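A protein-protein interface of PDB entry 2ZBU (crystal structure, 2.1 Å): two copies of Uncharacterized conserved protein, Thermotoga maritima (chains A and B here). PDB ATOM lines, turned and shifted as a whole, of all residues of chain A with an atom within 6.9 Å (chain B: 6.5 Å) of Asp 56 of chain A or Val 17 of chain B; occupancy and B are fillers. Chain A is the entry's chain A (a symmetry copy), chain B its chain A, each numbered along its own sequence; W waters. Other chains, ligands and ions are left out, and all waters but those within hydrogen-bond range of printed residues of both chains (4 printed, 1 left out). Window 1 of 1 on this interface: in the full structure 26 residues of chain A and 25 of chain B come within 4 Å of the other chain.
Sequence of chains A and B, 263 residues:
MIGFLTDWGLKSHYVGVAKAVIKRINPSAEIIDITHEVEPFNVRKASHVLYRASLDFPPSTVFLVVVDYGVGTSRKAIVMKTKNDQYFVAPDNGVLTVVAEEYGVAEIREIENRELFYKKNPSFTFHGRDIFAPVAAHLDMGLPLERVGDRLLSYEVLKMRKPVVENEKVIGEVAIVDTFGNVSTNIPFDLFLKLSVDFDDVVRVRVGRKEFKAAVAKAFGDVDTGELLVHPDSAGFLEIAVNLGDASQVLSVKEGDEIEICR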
ATOM      1  N   MET A   1     -40.807 -21.621  -9.923  1.00  0.00           N
ATOM      2  CA  MET A   1     -40.005 -20.955  -8.862  1.00  0.00           C
ATOM      3  C   MET A   1     -39.999 -19.441  -9.016  1.00  0.00           C
ATOM      4  O   MET A   1     -40.322 -18.901 -10.077  1.00  0.00           O
ATOM      5  CB  MET A   1     -38.561 -21.488  -8.836  1.00  0.00           C
ATOM      6  CG  MET A   1     -37.704 -21.233 -10.075  1.00  0.00           C
ATOM      7  SD  MET A   1     -35.933 -22.078  -9.914  1.00  0.00           S
ATOM      8  CE  MET A   1     -36.387 -23.899 -10.271  1.00  0.00           C
ATOM      9  N   ILE A  32     -36.042 -18.494  -4.667  1.00  0.00           N
ATOM     10  CA  ILE A  32     -34.606 -18.513  -4.812  1.00  0.00           C
ATOM     11  C   ILE A  32     -34.089 -17.083  -4.890  1.00  0.00           C
ATOM     12  O   ILE A  32     -34.459 -16.325  -5.787  1.00  0.00           O
ATOM     13  CB  ILE A  32     -34.189 -19.301  -6.063  1.00  0.00           C
ATOM     14  CG1 ILE A  32     -34.663 -20.754  -5.925  1.00  0.00           C
ATOM     15  CG2 ILE A  32     -32.675 -19.223  -6.244  1.00  0.00           C
ATOM     16  CD1 ILE A  32     -34.159 -21.680  -6.999  1.00  0.00           C
ATOM     17  N   ASP A  33     -33.244 -16.727  -3.924  1.00  0.00           N
ATOM     18  CA  ASP A  33     -32.648 -15.405  -3.854  1.00  0.00           C
ATOM     19  C   ASP A  33     -31.567 -15.210  -4.915  1.00  0.00           C
ATOM     20  O   ASP A  33     -30.605 -15.979  -4.997  1.00  0.00           O
ATOM     21  CB  ASP A  33     -32.038 -15.193  -2.464  1.00  0.00           C
ATOM     22  CG  ASP A  33     -33.090 -15.170  -1.364  1.00  0.00           C
ATOM     23  OD1 ASP A  33     -32.773 -15.622  -0.256  1.00  0.00           O
ATOM     24  OD2 ASP A  33     -34.225 -14.688  -1.617  1.00  0.00           O
ATOM     25  N   ILE A  34     -31.730 -14.191  -5.745  1.00  0.00           N
ATOM     26  CA  ILE A  34     -30.707 -13.919  -6.736  1.00  0.00           C
ATOM     27  C   ILE A  34     -29.668 -13.111  -5.964  1.00  0.00           C
ATOM     28  O   ILE A  34     -28.480 -13.415  -6.006  1.00  0.00           O
ATOM     29  CB  ILE A  34     -31.294 -13.180  -7.933  1.00  0.00           C
ATOM     30  CG1 ILE A  34     -32.268 -14.130  -8.656  1.00  0.00           C
ATOM     31  CG2 ILE A  34     -30.186 -12.734  -8.862  1.00  0.00           C
ATOM     32  CD1 ILE A  34     -33.089 -13.510  -9.794  1.00  0.00           C
ATOM     33  N   TYR A  51     -30.805  -9.825 -15.679  1.00  0.00           N
ATOM     34  CA  TYR A  51     -30.620 -10.514 -16.947  1.00  0.00           C
ATOM     35  C   TYR A  51     -29.655 -11.686 -16.815  1.00  0.00           C
ATOM     36  O   TYR A  51     -29.976 -12.814 -17.186  1.00  0.00           O
ATOM     37  CB  TYR A  51     -30.081  -9.556 -18.020  1.00  0.00           C
ATOM     38  CG  TYR A  51     -29.649 -10.281 -19.274  1.00  0.00           C
ATOM     39  CD1 TYR A  51     -30.559 -11.056 -19.993  1.00  0.00           C
ATOM     40  CD2 TYR A  51     -28.320 -10.235 -19.719  1.00  0.00           C
ATOM     41  CE1 TYR A  51     -30.169 -11.776 -21.120  1.00  0.00           C
ATOM     42  CE2 TYR A  51     -27.918 -10.949 -20.851  1.00  0.00           C
ATOM     43  CZ  TYR A  51     -28.851 -11.722 -21.544  1.00  0.00           C
ATOM     44  OH  TYR A  51     -28.479 -12.464 -22.644  1.00  0.00           O
ATOM     45  N   ARG A  52     -28.468 -11.417 -16.286  1.00  0.00           N
ATOM     46  CA  ARG A  52     -27.453 -12.457 -16.151  1.00  0.00           C
ATOM     47  C   ARG A  52     -27.914 -13.664 -15.349  1.00  0.00           C
ATOM     48  O   ARG A  52     -27.636 -14.806 -15.718  1.00  0.00           O
ATOM     49  CB  ARG A  52     -26.172 -11.842 -15.581  1.00  0.00           C
ATOM     50  CG  ARG A  52     -25.607 -10.807 -16.544  1.00  0.00           C
ATOM     51  CD  ARG A  52     -24.371 -10.076 -16.055  1.00  0.00           C
ATOM     52  NE  ARG A  52     -24.062  -9.022 -17.016  1.00  0.00           N
ATOM     53  CZ  ARG A  52     -22.843  -8.581 -17.310  1.00  0.00           C
ATOM     54  NH1 ARG A  52     -21.776  -9.092 -16.714  1.00  0.00           N
ATOM     55  NH2 ARG A  52     -22.695  -7.641 -18.234  1.00  0.00           N
ATOM     56  N   ALA A  53     -28.659 -13.421 -14.276  1.00  0.00           N
ATOM     57  CA  ALA A  53     -29.161 -14.517 -13.464  1.00  0.00           C
ATOM     58  C   ALA A  53     -30.293 -15.257 -14.174  1.00  0.00           C
ATOM     59  O   ALA A  53     -30.383 -16.479 -14.101  1.00  0.00           O
ATOM     60  CB  ALA A  53     -29.648 -13.994 -12.115  1.00  0.00           C
ATOM     61  N   SER A  54     -31.150 -14.522 -14.875  1.00  0.00           N
ATOM     62  CA  SER A  54     -32.290 -15.153 -15.544  1.00  0.00           C
ATOM     63  C   SER A  54     -31.900 -16.239 -16.556  1.00  0.00           C
ATOM     64  O   SER A  54     -32.670 -17.161 -16.805  1.00  0.00           O
ATOM     65  CB  SER A  54     -33.155 -14.094 -16.230  1.00  0.00           C
ATOM     66  OG  SER A  54     -32.505 -13.596 -17.380  1.00  0.00           O
ATOM     67  N   LEU A  55     -30.710 -16.115 -17.141  1.00  0.00           N
ATOM     68  CA  LEU A  55     -30.214 -17.081 -18.118  1.00  0.00           C
ATOM     69  C   LEU A  55     -30.145 -18.511 -17.583  1.00  0.00           C
ATOM     70  O   LEU A  55     -30.139 -19.467 -18.361  1.00  0.00           O
ATOM     71  CB  LEU A  55     -28.821 -16.657 -18.607  1.00  0.00           C
ATOM     72  CG  LEU A  55     -28.814 -15.332 -19.375  1.00  0.00           C
ATOM     73  CD1 LEU A  55     -27.404 -14.828 -19.552  1.00  0.00           C
ATOM     74  CD2 LEU A  55     -29.511 -15.533 -20.721  1.00  0.00           C
ATOM     75  N   ASP A  56     -30.066 -18.658 -16.264  1.00  0.00           N
ATOM     76  CA  ASP A  56     -29.993 -19.984 -15.665  1.00  0.00           C
ATOM     77  C   ASP A  56     -31.275 -20.406 -14.957  1.00  0.00           C
ATOM     78  O   ASP A  56     -31.303 -21.441 -14.291  1.00  0.00           O
ATOM     79  CB  ASP A  56     -28.810 -20.065 -14.695  1.00  0.00           C
ATOM     80  CG  ASP A  56     -27.479 -19.958 -15.410  1.00  0.00           C
ATOM     81  OD1 ASP A  56     -27.253 -20.744 -16.352  1.00  0.00           O
ATOM     82  OD2 ASP A  56     -26.666 -19.094 -15.034  1.00  0.00           O
ATOM     83  N   PHE A  57     -32.320 -19.592 -15.079  1.00  0.00           N
ATOM     84  CA  PHE A  57     -33.608 -19.928 -14.479  1.00  0.00           C
ATOM     85  C   PHE A  57     -34.422 -20.510 -15.622  1.00  0.00           C
ATOM     86  O   PHE A  57     -34.269 -20.116 -16.780  1.00  0.00           O
ATOM     87  CB  PHE A  57     -34.304 -18.685 -13.885  1.00  0.00           C
ATOM     88  CG  PHE A  57     -33.872 -18.367 -12.475  1.00  0.00           C
ATOM     89  CD1 PHE A  57     -34.652 -18.761 -11.384  1.00  0.00           C
ATOM     90  CD2 PHE A  57     -32.672 -17.690 -12.234  1.00  0.00           C
ATOM     91  CE1 PHE A  57     -34.238 -18.482 -10.058  1.00  0.00           C
ATOM     92  CE2 PHE A  57     -32.250 -17.410 -10.926  1.00  0.00           C
ATOM     93  CZ  PHE A  57     -33.042 -17.809  -9.833  1.00  0.00           C
ATOM     94  N   PRO A  58     -35.290 -21.472 -15.317  1.00  0.00           N
ATOM     95  CA  PRO A  58     -36.080 -22.059 -16.398  1.00  0.00           C
ATOM     96  C   PRO A  58     -37.168 -21.138 -16.924  1.00  0.00           C
ATOM     97  O   PRO A  58     -37.445 -20.084 -16.347  1.00  0.00           O
ATOM     98  CB  PRO A  58     -36.658 -23.301 -15.747  1.00  0.00           C
ATOM     99  CG  PRO A  58     -36.896 -22.820 -14.325  1.00  0.00           C
ATOM    100  CD  PRO A  58     -35.629 -22.070 -14.014  1.00  0.00           C
ATOM    101  N   THR A  61     -40.378 -18.963 -15.023  1.00  0.00           N
ATOM    102  CA  THR A  61     -39.915 -18.534 -13.716  1.00  0.00           C
ATOM    103  C   THR A  61     -40.546 -17.151 -13.505  1.00  0.00           C
ATOM    104  O   THR A  61     -40.660 -16.365 -14.458  1.00  0.00           O
ATOM    105  CB  THR A  61     -38.379 -18.375 -13.680  1.00  0.00           C
ATOM    106  OG1 THR A  61     -37.769 -19.667 -13.561  1.00  0.00           O
ATOM    107  CG2 THR A  61     -37.956 -17.483 -12.513  1.00  0.00           C
ATOM    108  N   PHE A  63     -40.026 -13.725 -11.717  1.00  0.00           N
ATOM    109  CA  PHE A  63     -39.026 -12.917 -11.038  1.00  0.00           C
ATOM    110  C   PHE A  63     -39.669 -11.783 -10.235  1.00  0.00           C
ATOM    111  O   PHE A  63     -40.550 -11.069 -10.718  1.00  0.00           O
ATOM    112  CB  PHE A  63     -38.013 -12.372 -12.059  1.00  0.00           C
ATOM    113  CG  PHE A  63     -37.156 -13.445 -12.701  1.00  0.00           C
ATOM    114  CD1 PHE A  63     -35.969 -13.867 -12.092  1.00  0.00           C
ATOM    115  CD2 PHE A  63     -37.538 -14.037 -13.905  1.00  0.00           C
ATOM    116  CE1 PHE A  63     -35.172 -14.871 -12.687  1.00  0.00           C
ATOM    117  CE2 PHE A  63     -36.752 -15.040 -14.507  1.00  0.00           C
ATOM    118  CZ  PHE A  63     -35.568 -15.454 -13.893  1.00  0.00           C
ATOM    119  N   GLN A  86     -40.519 -16.021 -19.648  1.00  0.00           N
ATOM    120  CA  GLN A  86     -40.261 -15.736 -18.241  1.00  0.00           C
ATOM    121  C   GLN A  86     -41.149 -14.544 -17.863  1.00  0.00           C
ATOM    122  O   GLN A  86     -41.616 -13.812 -18.740  1.00  0.00           O
ATOM    123  CB  GLN A  86     -38.767 -15.460 -17.989  1.00  0.00           C
ATOM    124  CG  GLN A  86     -37.901 -16.737 -18.121  1.00  0.00           C
ATOM    125  CD  GLN A  86     -36.433 -16.525 -17.731  1.00  0.00           C
ATOM    126  OE1 GLN A  86     -35.859 -15.487 -18.028  1.00  0.00           O
ATOM    127  NE2 GLN A  86     -35.823 -17.526 -17.076  1.00  0.00           N
ATOM    128  N   TYR A 103     -34.386 -10.403 -24.335  1.00  0.00           N
ATOM    129  CA  TYR A 103     -35.387 -11.440 -24.583  1.00  0.00           C
ATOM    130  C   TYR A 103     -36.564 -11.005 -25.461  1.00  0.00           C
ATOM    131  O   TYR A 103     -37.209 -11.846 -26.090  1.00  0.00           O
ATOM    132  CB  TYR A 103     -35.972 -11.968 -23.259  1.00  0.00           C
ATOM    133  CG  TYR A 103     -34.996 -12.645 -22.314  1.00  0.00           C
ATOM    134  CD1 TYR A 103     -34.019 -13.525 -22.786  1.00  0.00           C
ATOM    135  CD2 TYR A 103     -35.090 -12.447 -20.939  1.00  0.00           C
ATOM    136  CE1 TYR A 103     -33.159 -14.193 -21.899  1.00  0.00           C
ATOM    137  CE2 TYR A 103     -34.239 -13.106 -20.049  1.00  0.00           C
ATOM    138  CZ  TYR A 103     -33.277 -13.976 -20.535  1.00  0.00           C
ATOM    139  OH  TYR A 103     -32.437 -14.615 -19.662  1.00  0.00           O
ATOM    140  N   SER A 234     -19.206 -16.454 -16.676  1.00  0.00           N
ATOM    141  CA  SER A 234     -20.248 -17.469 -16.771  1.00  0.00           C
ATOM    142  C   SER A 234     -21.486 -17.105 -17.590  1.00  0.00           C
ATOM    143  O   SER A 234     -22.241 -17.991 -17.976  1.00  0.00           O
ATOM    144  CB  SER A 234     -20.670 -17.929 -15.368  1.00  0.00           C
ATOM    145  OG  SER A 234     -21.178 -16.848 -14.612  1.00  0.00           O
ATOM    146  N   ALA A 235     -21.696 -15.816 -17.852  1.00  0.00           N
ATOM    147  CA  ALA A 235     -22.845 -15.363 -18.639  1.00  0.00           C
ATOM    148  C   ALA A 235     -22.488 -14.984 -20.089  1.00  0.00           C
ATOM    149  O   ALA A 235     -23.339 -14.481 -20.831  1.00  0.00           O
ATOM    150  CB  ALA A 235     -23.522 -14.173 -17.947  1.00  0.00           C
ATOM    151  N   TRP B   8     -18.117 -17.772  -2.596  1.00  0.00           N
ATOM    152  CA  TRP B   8     -18.742 -16.878  -3.577  1.00  0.00           C
ATOM    153  C   TRP B   8     -19.389 -15.617  -3.013  1.00  0.00           C
ATOM    154  O   TRP B   8     -19.582 -14.637  -3.742  1.00  0.00           O
ATOM    155  CB  TRP B   8     -19.816 -17.615  -4.375  1.00  0.00           C
ATOM    156  CG  TRP B   8     -19.411 -18.931  -4.982  1.00  0.00           C
ATOM    157  CD1 TRP B   8     -18.150 -19.451  -5.078  1.00  0.00           C
ATOM    158  CD2 TRP B   8     -20.289 -19.897  -5.564  1.00  0.00           C
ATOM    159  NE1 TRP B   8     -18.190 -20.684  -5.681  1.00  0.00           N
ATOM    160  CE2 TRP B   8     -19.491 -20.984  -5.990  1.00  0.00           C
ATOM    161  CE3 TRP B   8     -21.679 -19.954  -5.764  1.00  0.00           C
ATOM    162  CZ2 TRP B   8     -20.038 -22.119  -6.605  1.00  0.00           C
ATOM    163  CZ3 TRP B   8     -22.218 -21.074  -6.372  1.00  0.00           C
ATOM    164  CH2 TRP B   8     -21.396 -22.146  -6.786  1.00  0.00           C
ATOM    165  N   HIS B  13     -24.983 -12.998  -7.697  1.00  0.00           N
ATOM    166  CA  HIS B  13     -26.087 -13.874  -8.062  1.00  0.00           C
ATOM    167  C   HIS B  13     -25.583 -15.322  -8.228  1.00  0.00           C
ATOM    168  O   HIS B  13     -26.357 -16.211  -8.554  1.00  0.00           O
ATOM    169  CB  HIS B  13     -26.703 -13.418  -9.389  1.00  0.00           C
ATOM    170  CG  HIS B  13     -25.730 -13.406 -10.528  1.00  0.00           C
ATOM    171  ND1 HIS B  13     -24.798 -12.404 -10.700  1.00  0.00           N
ATOM    172  CD2 HIS B  13     -25.519 -14.291 -11.530  1.00  0.00           C
ATOM    173  CE1 HIS B  13     -24.057 -12.672 -11.760  1.00  0.00           C
ATOM    174  NE2 HIS B  13     -24.474 -13.811 -12.283  1.00  0.00           N
ATOM    175  N   TYR B  14     -24.293 -15.560  -8.002  1.00  0.00           N
ATOM    176  CA  TYR B  14     -23.739 -16.912  -8.171  1.00  0.00           C
ATOM    177  C   TYR B  14     -24.412 -18.008  -7.342  1.00  0.00           C
ATOM    178  O   TYR B  14     -24.784 -19.058  -7.866  1.00  0.00           O
ATOM    179  CB  TYR B  14     -22.240 -16.930  -7.869  1.00  0.00           C
ATOM    180  CG  TYR B  14     -21.412 -15.912  -8.622  1.00  0.00           C
ATOM    181  CD1 TYR B  14     -21.644 -15.644  -9.976  1.00  0.00           C
ATOM    182  CD2 TYR B  14     -20.352 -15.257  -7.993  1.00  0.00           C
ATOM    183  CE1 TYR B  14     -20.832 -14.751 -10.683  1.00  0.00           C
ATOM    184  CE2 TYR B  14     -19.541 -14.368  -8.687  1.00  0.00           C
ATOM    185  CZ  TYR B  14     -19.781 -14.121 -10.028  1.00  0.00           C
ATOM    186  OH  TYR B  14     -18.945 -13.262 -10.710  1.00  0.00           O
ATOM    187  N   VAL B  15     -24.541 -17.786  -6.041  1.00  0.00           N
ATOM    188  CA  VAL B  15     -25.169 -18.786  -5.200  1.00  0.00           C
ATOM    189  C   VAL B  15     -26.568 -19.081  -5.757  1.00  0.00           C
ATOM    190  O   VAL B  15     -26.956 -20.236  -5.916  1.00  0.00           O
ATOM    191  CB  VAL B  15     -25.275 -18.299  -3.737  1.00  0.00           C
ATOM    192  CG1 VAL B  15     -26.173 -19.253  -2.921  1.00  0.00           C
ATOM    193  CG2 VAL B  15     -23.876 -18.250  -3.102  1.00  0.00           C
ATOM    194  N   GLY B  16     -27.306 -18.023  -6.070  1.00  0.00           N
ATOM    195  CA  GLY B  16     -28.653 -18.178  -6.591  1.00  0.00           C
ATOM    196  C   GLY B  16     -28.805 -19.013  -7.855  1.00  0.00           C
ATOM    197  O   GLY B  16     -29.703 -19.864  -7.932  1.00  0.00           O
ATOM    198  N   VAL B  17     -27.958 -18.768  -8.858  1.00  0.00           N
ATOM    199  CA  VAL B  17     -28.077 -19.535 -10.079  1.00  0.00           C
ATOM    200  C   VAL B  17     -27.699 -20.982  -9.819  1.00  0.00           C
ATOM    201  O   VAL B  17     -28.240 -21.872 -10.451  1.00  0.00           O
ATOM    202  CB  VAL B  17     -27.233 -18.940 -11.268  1.00  0.00           C
ATOM    203  CG1 VAL B  17     -27.721 -17.535 -11.587  1.00  0.00           C
ATOM    204  CG2 VAL B  17     -25.754 -18.923 -10.940  1.00  0.00           C
ATOM    205  N   ALA B  18     -26.786 -21.225  -8.879  1.00  0.00           N
ATOM    206  CA  ALA B  18     -26.415 -22.601  -8.558  1.00  0.00           C
ATOM    207  C   ALA B  18     -27.638 -23.323  -7.947  1.00  0.00           C
ATOM    208  O   ALA B  18     -27.933 -24.476  -8.286  1.00  0.00           O
ATOM    209  CB  ALA B  18     -25.237 -22.625  -7.558  1.00  0.00           C
ATOM    210  N   LYS B  19     -28.337 -22.643  -7.040  1.00  0.00           N
ATOM    211  CA  LYS B  19     -29.509 -23.225  -6.403  1.00  0.00           C
ATOM    212  C   LYS B  19     -30.625 -23.477  -7.419  1.00  0.00           C
ATOM    213  O   LYS B  19     -31.345 -24.471  -7.317  1.00  0.00           O
ATOM    214  CB  LYS B  19     -30.022 -22.316  -5.280  1.00  0.00           C
ATOM    215  CG  LYS B  19     -29.087 -22.261  -4.059  1.00  0.00           C
ATOM    216  CD  LYS B  19     -29.724 -21.476  -2.919  1.00  0.00           C
ATOM    217  CE  LYS B  19     -28.817 -21.457  -1.684  1.00  0.00           C
ATOM    218  NZ  LYS B  19     -29.437 -20.726  -0.564  1.00  0.00           N
ATOM    219  N   ALA B  20     -30.763 -22.587  -8.402  1.00  0.00           N
ATOM    220  CA  ALA B  20     -31.798 -22.765  -9.418  1.00  0.00           C
ATOM    221  C   ALA B  20     -31.485 -24.007 -10.264  1.00  0.00           C
ATOM    222  O   ALA B  20     -32.397 -24.737 -10.663  1.00  0.00           O
ATOM    223  CB  ALA B  20     -31.889 -21.534 -10.303  1.00  0.00           C
ATOM    224  N   VAL B  21     -30.202 -24.242 -10.544  1.00  0.00           N
ATOM    225  CA  VAL B  21     -29.806 -25.424 -11.316  1.00  0.00           C
ATOM    226  C   VAL B  21     -30.177 -26.689 -10.530  1.00  0.00           C
ATOM    227  O   VAL B  21     -30.748 -27.636 -11.076  1.00  0.00           O
ATOM    228  CB  VAL B  21     -28.287 -25.424 -11.598  1.00  0.00           C
ATOM    229  CG1 VAL B  21     -27.841 -26.789 -12.189  1.00  0.00           C
ATOM    230  CG2 VAL B  21     -27.952 -24.303 -12.578  1.00  0.00           C
ATOM    231  N   ILE B  22     -29.848 -26.700  -9.242  1.00  0.00           N
ATOM    232  CA  ILE B  22     -30.172 -27.844  -8.399  1.00  0.00           C
ATOM    233  C   ILE B  22     -31.682 -28.088  -8.404  1.00  0.00           C
ATOM    234  O   ILE B  22     -32.144 -29.213  -8.631  1.00  0.00           O
ATOM    235  CB  ILE B  22     -29.687 -27.612  -6.940  1.00  0.00           C
ATOM    236  CG1 ILE B  22     -28.155 -27.542  -6.913  1.00  0.00           C
ATOM    237  CG2 ILE B  22     -30.215 -28.718  -6.024  1.00  0.00           C
ATOM    238  CD1 ILE B  22     -27.578 -27.093  -5.568  1.00  0.00           C
ATOM    239  N   ARG B  24     -33.879 -27.200 -10.582  1.00  0.00           N
ATOM    240  CA  ARG B  24     -34.395 -27.584 -11.895  1.00  0.00           C
ATOM    241  C   ARG B  24     -34.236 -29.098 -12.043  1.00  0.00           C
ATOM    242  O   ARG B  24     -35.106 -29.771 -12.574  1.00  0.00           O
ATOM    243  CB  ARG B  24     -33.625 -26.866 -13.020  1.00  0.00           C
ATOM    244  CG  ARG B  24     -33.810 -25.348 -13.020  1.00  0.00           C
ATOM    245  CD  ARG B  24     -32.981 -24.655 -14.106  1.00  0.00           C
ATOM    246  NE  ARG B  24     -33.506 -24.931 -15.436  1.00  0.00           N
ATOM    247  CZ  ARG B  24     -33.058 -24.367 -16.555  1.00  0.00           C
ATOM    248  NH1 ARG B  24     -32.067 -23.489 -16.511  1.00  0.00           N
ATOM    249  NH2 ARG B  24     -33.608 -24.678 -17.719  1.00  0.00           N
ATOM    250  N   TYR B 118     -24.903 -29.621 -16.076  1.00  0.00           N
ATOM    251  CA  TYR B 118     -25.982 -28.671 -16.296  1.00  0.00           C
ATOM    252  C   TYR B 118     -26.004 -28.301 -17.778  1.00  0.00           C
ATOM    253  O   TYR B 118     -27.059 -28.280 -18.402  1.00  0.00           O
ATOM    254  CB  TYR B 118     -25.762 -27.413 -15.449  1.00  0.00           C
ATOM    255  CG  TYR B 118     -26.591 -26.213 -15.880  1.00  0.00           C
ATOM    256  CD1 TYR B 118     -27.971 -26.322 -16.096  1.00  0.00           C
ATOM    257  CD2 TYR B 118     -25.996 -24.959 -16.036  1.00  0.00           C
ATOM    258  CE1 TYR B 118     -28.735 -25.207 -16.457  1.00  0.00           C
ATOM    259  CE2 TYR B 118     -26.743 -23.842 -16.391  1.00  0.00           C
ATOM    260  CZ  TYR B 118     -28.110 -23.966 -16.601  1.00  0.00           C
ATOM    261  OH  TYR B 118     -28.838 -22.847 -16.940  1.00  0.00           O
ATOM    262  N   LYS B 119     -24.826 -28.029 -18.333  1.00  0.00           N
ATOM    263  CA  LYS B 119     -24.700 -27.641 -19.736  1.00  0.00           C
ATOM    264  C   LYS B 119     -23.761 -28.560 -20.498  1.00  0.00           C
ATOM    265  O   LYS B 119     -22.759 -29.031 -19.960  1.00  0.00           O
ATOM    266  CB  LYS B 119     -24.178 -26.200 -19.855  1.00  0.00           C
ATOM    267  CG  LYS B 119     -25.061 -25.183 -19.171  1.00  0.00           C
ATOM    268  CD  LYS B 119     -24.900 -23.779 -19.737  1.00  0.00           C
ATOM    269  CE  LYS B 119     -23.560 -23.168 -19.421  1.00  0.00           C
ATOM    270  NZ  LYS B 119     -23.528 -21.771 -19.927  1.00  0.00           N
ATOM    271  N   PHE B 126     -16.864 -21.469 -13.937  1.00  0.00           N
ATOM    272  CA  PHE B 126     -17.963 -21.644 -12.990  1.00  0.00           C
ATOM    273  C   PHE B 126     -18.468 -23.085 -12.957  1.00  0.00           C
ATOM    274  O   PHE B 126     -19.657 -23.336 -13.146  1.00  0.00           O
ATOM    275  CB  PHE B 126     -19.115 -20.674 -13.316  1.00  0.00           C
ATOM    276  CG  PHE B 126     -20.131 -20.501 -12.186  1.00  0.00           C
ATOM    277  CD1 PHE B 126     -19.897 -21.029 -10.919  1.00  0.00           C
ATOM    278  CD2 PHE B 126     -21.306 -19.787 -12.400  1.00  0.00           C
ATOM    279  CE1 PHE B 126     -20.819 -20.848  -9.878  1.00  0.00           C
ATOM    280  CE2 PHE B 126     -22.231 -19.599 -11.371  1.00  0.00           C
ATOM    281  CZ  PHE B 126     -21.988 -20.131 -10.108  1.00  0.00           C
ATOM    282  N   ARG B 129     -21.552 -24.206 -10.902  1.00  0.00           N
ATOM    283  CA  ARG B 129     -22.865 -24.252 -11.528  1.00  0.00           C
ATOM    284  C   ARG B 129     -23.046 -25.343 -12.576  1.00  0.00           C
ATOM    285  O   ARG B 129     -24.055 -26.048 -12.587  1.00  0.00           O
ATOM    286  CB  ARG B 129     -23.171 -22.914 -12.201  1.00  0.00           C
ATOM    287  CG  ARG B 129     -24.533 -22.873 -12.923  1.00  0.00           C
ATOM    288  CD  ARG B 129     -24.649 -21.637 -13.802  1.00  0.00           C
ATOM    289  NE  ARG B 129     -23.765 -21.755 -14.961  1.00  0.00           N
ATOM    290  CZ  ARG B 129     -23.433 -20.756 -15.769  1.00  0.00           C
ATOM    291  NH1 ARG B 129     -23.909 -19.532 -15.559  1.00  0.00           N
ATOM    292  NH2 ARG B 129     -22.615 -20.982 -16.791  1.00  0.00           N
ATOM    293  N   ASP B 130     -22.066 -25.474 -13.463  1.00  0.00           N
ATOM    294  CA  ASP B 130     -22.172 -26.424 -14.565  1.00  0.00           C
ATOM    295  C   ASP B 130     -21.839 -27.880 -14.309  1.00  0.00           C
ATOM    296  O   ASP B 130     -22.279 -28.757 -15.056  1.00  0.00           O
ATOM    297  CB  ASP B 130     -21.342 -25.909 -15.743  1.00  0.00           C
ATOM    298  CG  ASP B 130     -21.732 -24.498 -16.138  1.00  0.00           C
ATOM    299  OD1 ASP B 130     -22.885 -24.108 -15.837  1.00  0.00           O
ATOM    300  OD2 ASP B 130     -20.904 -23.784 -16.743  1.00  0.00           O
HETATM  301  O   HOH W   1     -23.482 -15.705 -14.612  1.00  0.00           O
HETATM  302  O   HOH W   2     -25.679 -16.716 -15.884  1.00  0.00           O
HETATM  303  O   HOH W   3     -21.286 -20.465 -19.519  1.00  0.00           O
HETATM  304  O   HOH W   4     -26.925 -15.492  -5.091  1.00  0.00           O
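The side-chain hydroxyl (OH) of Tyr 118 of chain B lies within hydrogen-bond range of the side-chain carboxylate (OD1) of Asp 56 of chain A (2.7 Å).
The guanidinium group (NH1) of Arg 129 of chain B is in salt-bridge range of the side-chain carboxylate (OD2) of Asp 56 of chain A, 2.8 Å away.
O of Ser 234 of chain A sits at hydrogen-bond distance from NH2 of Arg 129 of chain B, 3.2 Å away.
The backbone carbonyl oxygen (O) of Asp 56 of chain A lies within hydrogen-bond range of the guanidinium group (NH1) of Arg 24 of chain B (3.1 Å).
The guanidinium group (NE) of Arg 129 of chain B is in salt-bridge range of the side-chain carboxylate (OD1) of Asp 130 of chain B, at 2.7 Å.
The guanidinium group of Arg 24 of chain B sits at hydrogen-bond distance from the side-chain hydroxyl of Tyr 118 of chain B (3.3 Å).
Among the printed residues, pairs that only touch across the chains: Ile 32 of chain A with Gly 16 of chain B (3.5 Å), Ile 32 of chain A with Lys 19 of chain B (3.98 Å), Ile 32 of chain A with Ala 20 of chain B (3.6 Å), Asp 33 of chain A with Gly 16 of chain B (3.3 Å), Ile 34 of chain A with His 13 of chain B (3.2 Å), Ala 53 of chain A with Val 17 of chain B (3.8 Å), Leu 55 of chain A with Tyr 118 of chain B (3.9 Å), Asp 56 of chain A with Val 17 of chain B (3.8 Å), Phe 57 of chain A with Ala 20 of chain B (3.9 Å), Phe 57 of chain A with Arg 24 of chain B (3.9 Å), Pro 58 of chain A with Arg 24 of chain B (3.6 Å) and Ser 234 of chain A with Phe 126 of chain B (3.6 Å).
Of the printed residues of chain B, Asp 33 of chain A touches Gly 16 (3.3 Å).
Ser 54 of chain A touches none of the printed residues of chain B.
Printed residues of chain A within 4 Å of His 13 of chain B: Ile 34 (3.2 Å).
Val 17 of chain B touches just these residues of chain A: Ala 53 and Asp 56.
Of the printed residues of chain A, Lys 19 of chain B touches Ile 32.
Printed residues of chain A within 4 Å of Tyr 118 of chain B: Leu 55 and Asp 56.
The nearest residue of chain A that does not touch Val 17 of chain B is Phe 57 of chain A (4.6 Å).
Of the 18 printed residues of chain A, 9 touch a printed residue of chain B.
Hydrophobic or aromatic side chains of chain A that line the printed part of chain B: Ile 32, Ile 34, Phe 57 and Pro 58.
Printed residues of chain B that touch a printed residue of chain A: His 13, Gly 16, Val 17, Lys 19, Ala 20, Arg 24, Tyr 118, Phe 126 and Arg 129.
No position is printed for both chains.
Water W1 bridges the side-chain hydroxyl of Ser 234 of chain A (2.6 Å) and a ring nitrogen (NE2) of His 13 of chain B (3.2 Å).
Water W3 lies within hydrogen-bond range of the side-chain amino group (NZ) of Lys 119 of chain B (2.6 Å), the backbone carbonyl oxygen (O) of Ser 234 of chain A (3.1 Å) and the guanidinium group (NH2) of Arg 129 of chain B (3.1 Å).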
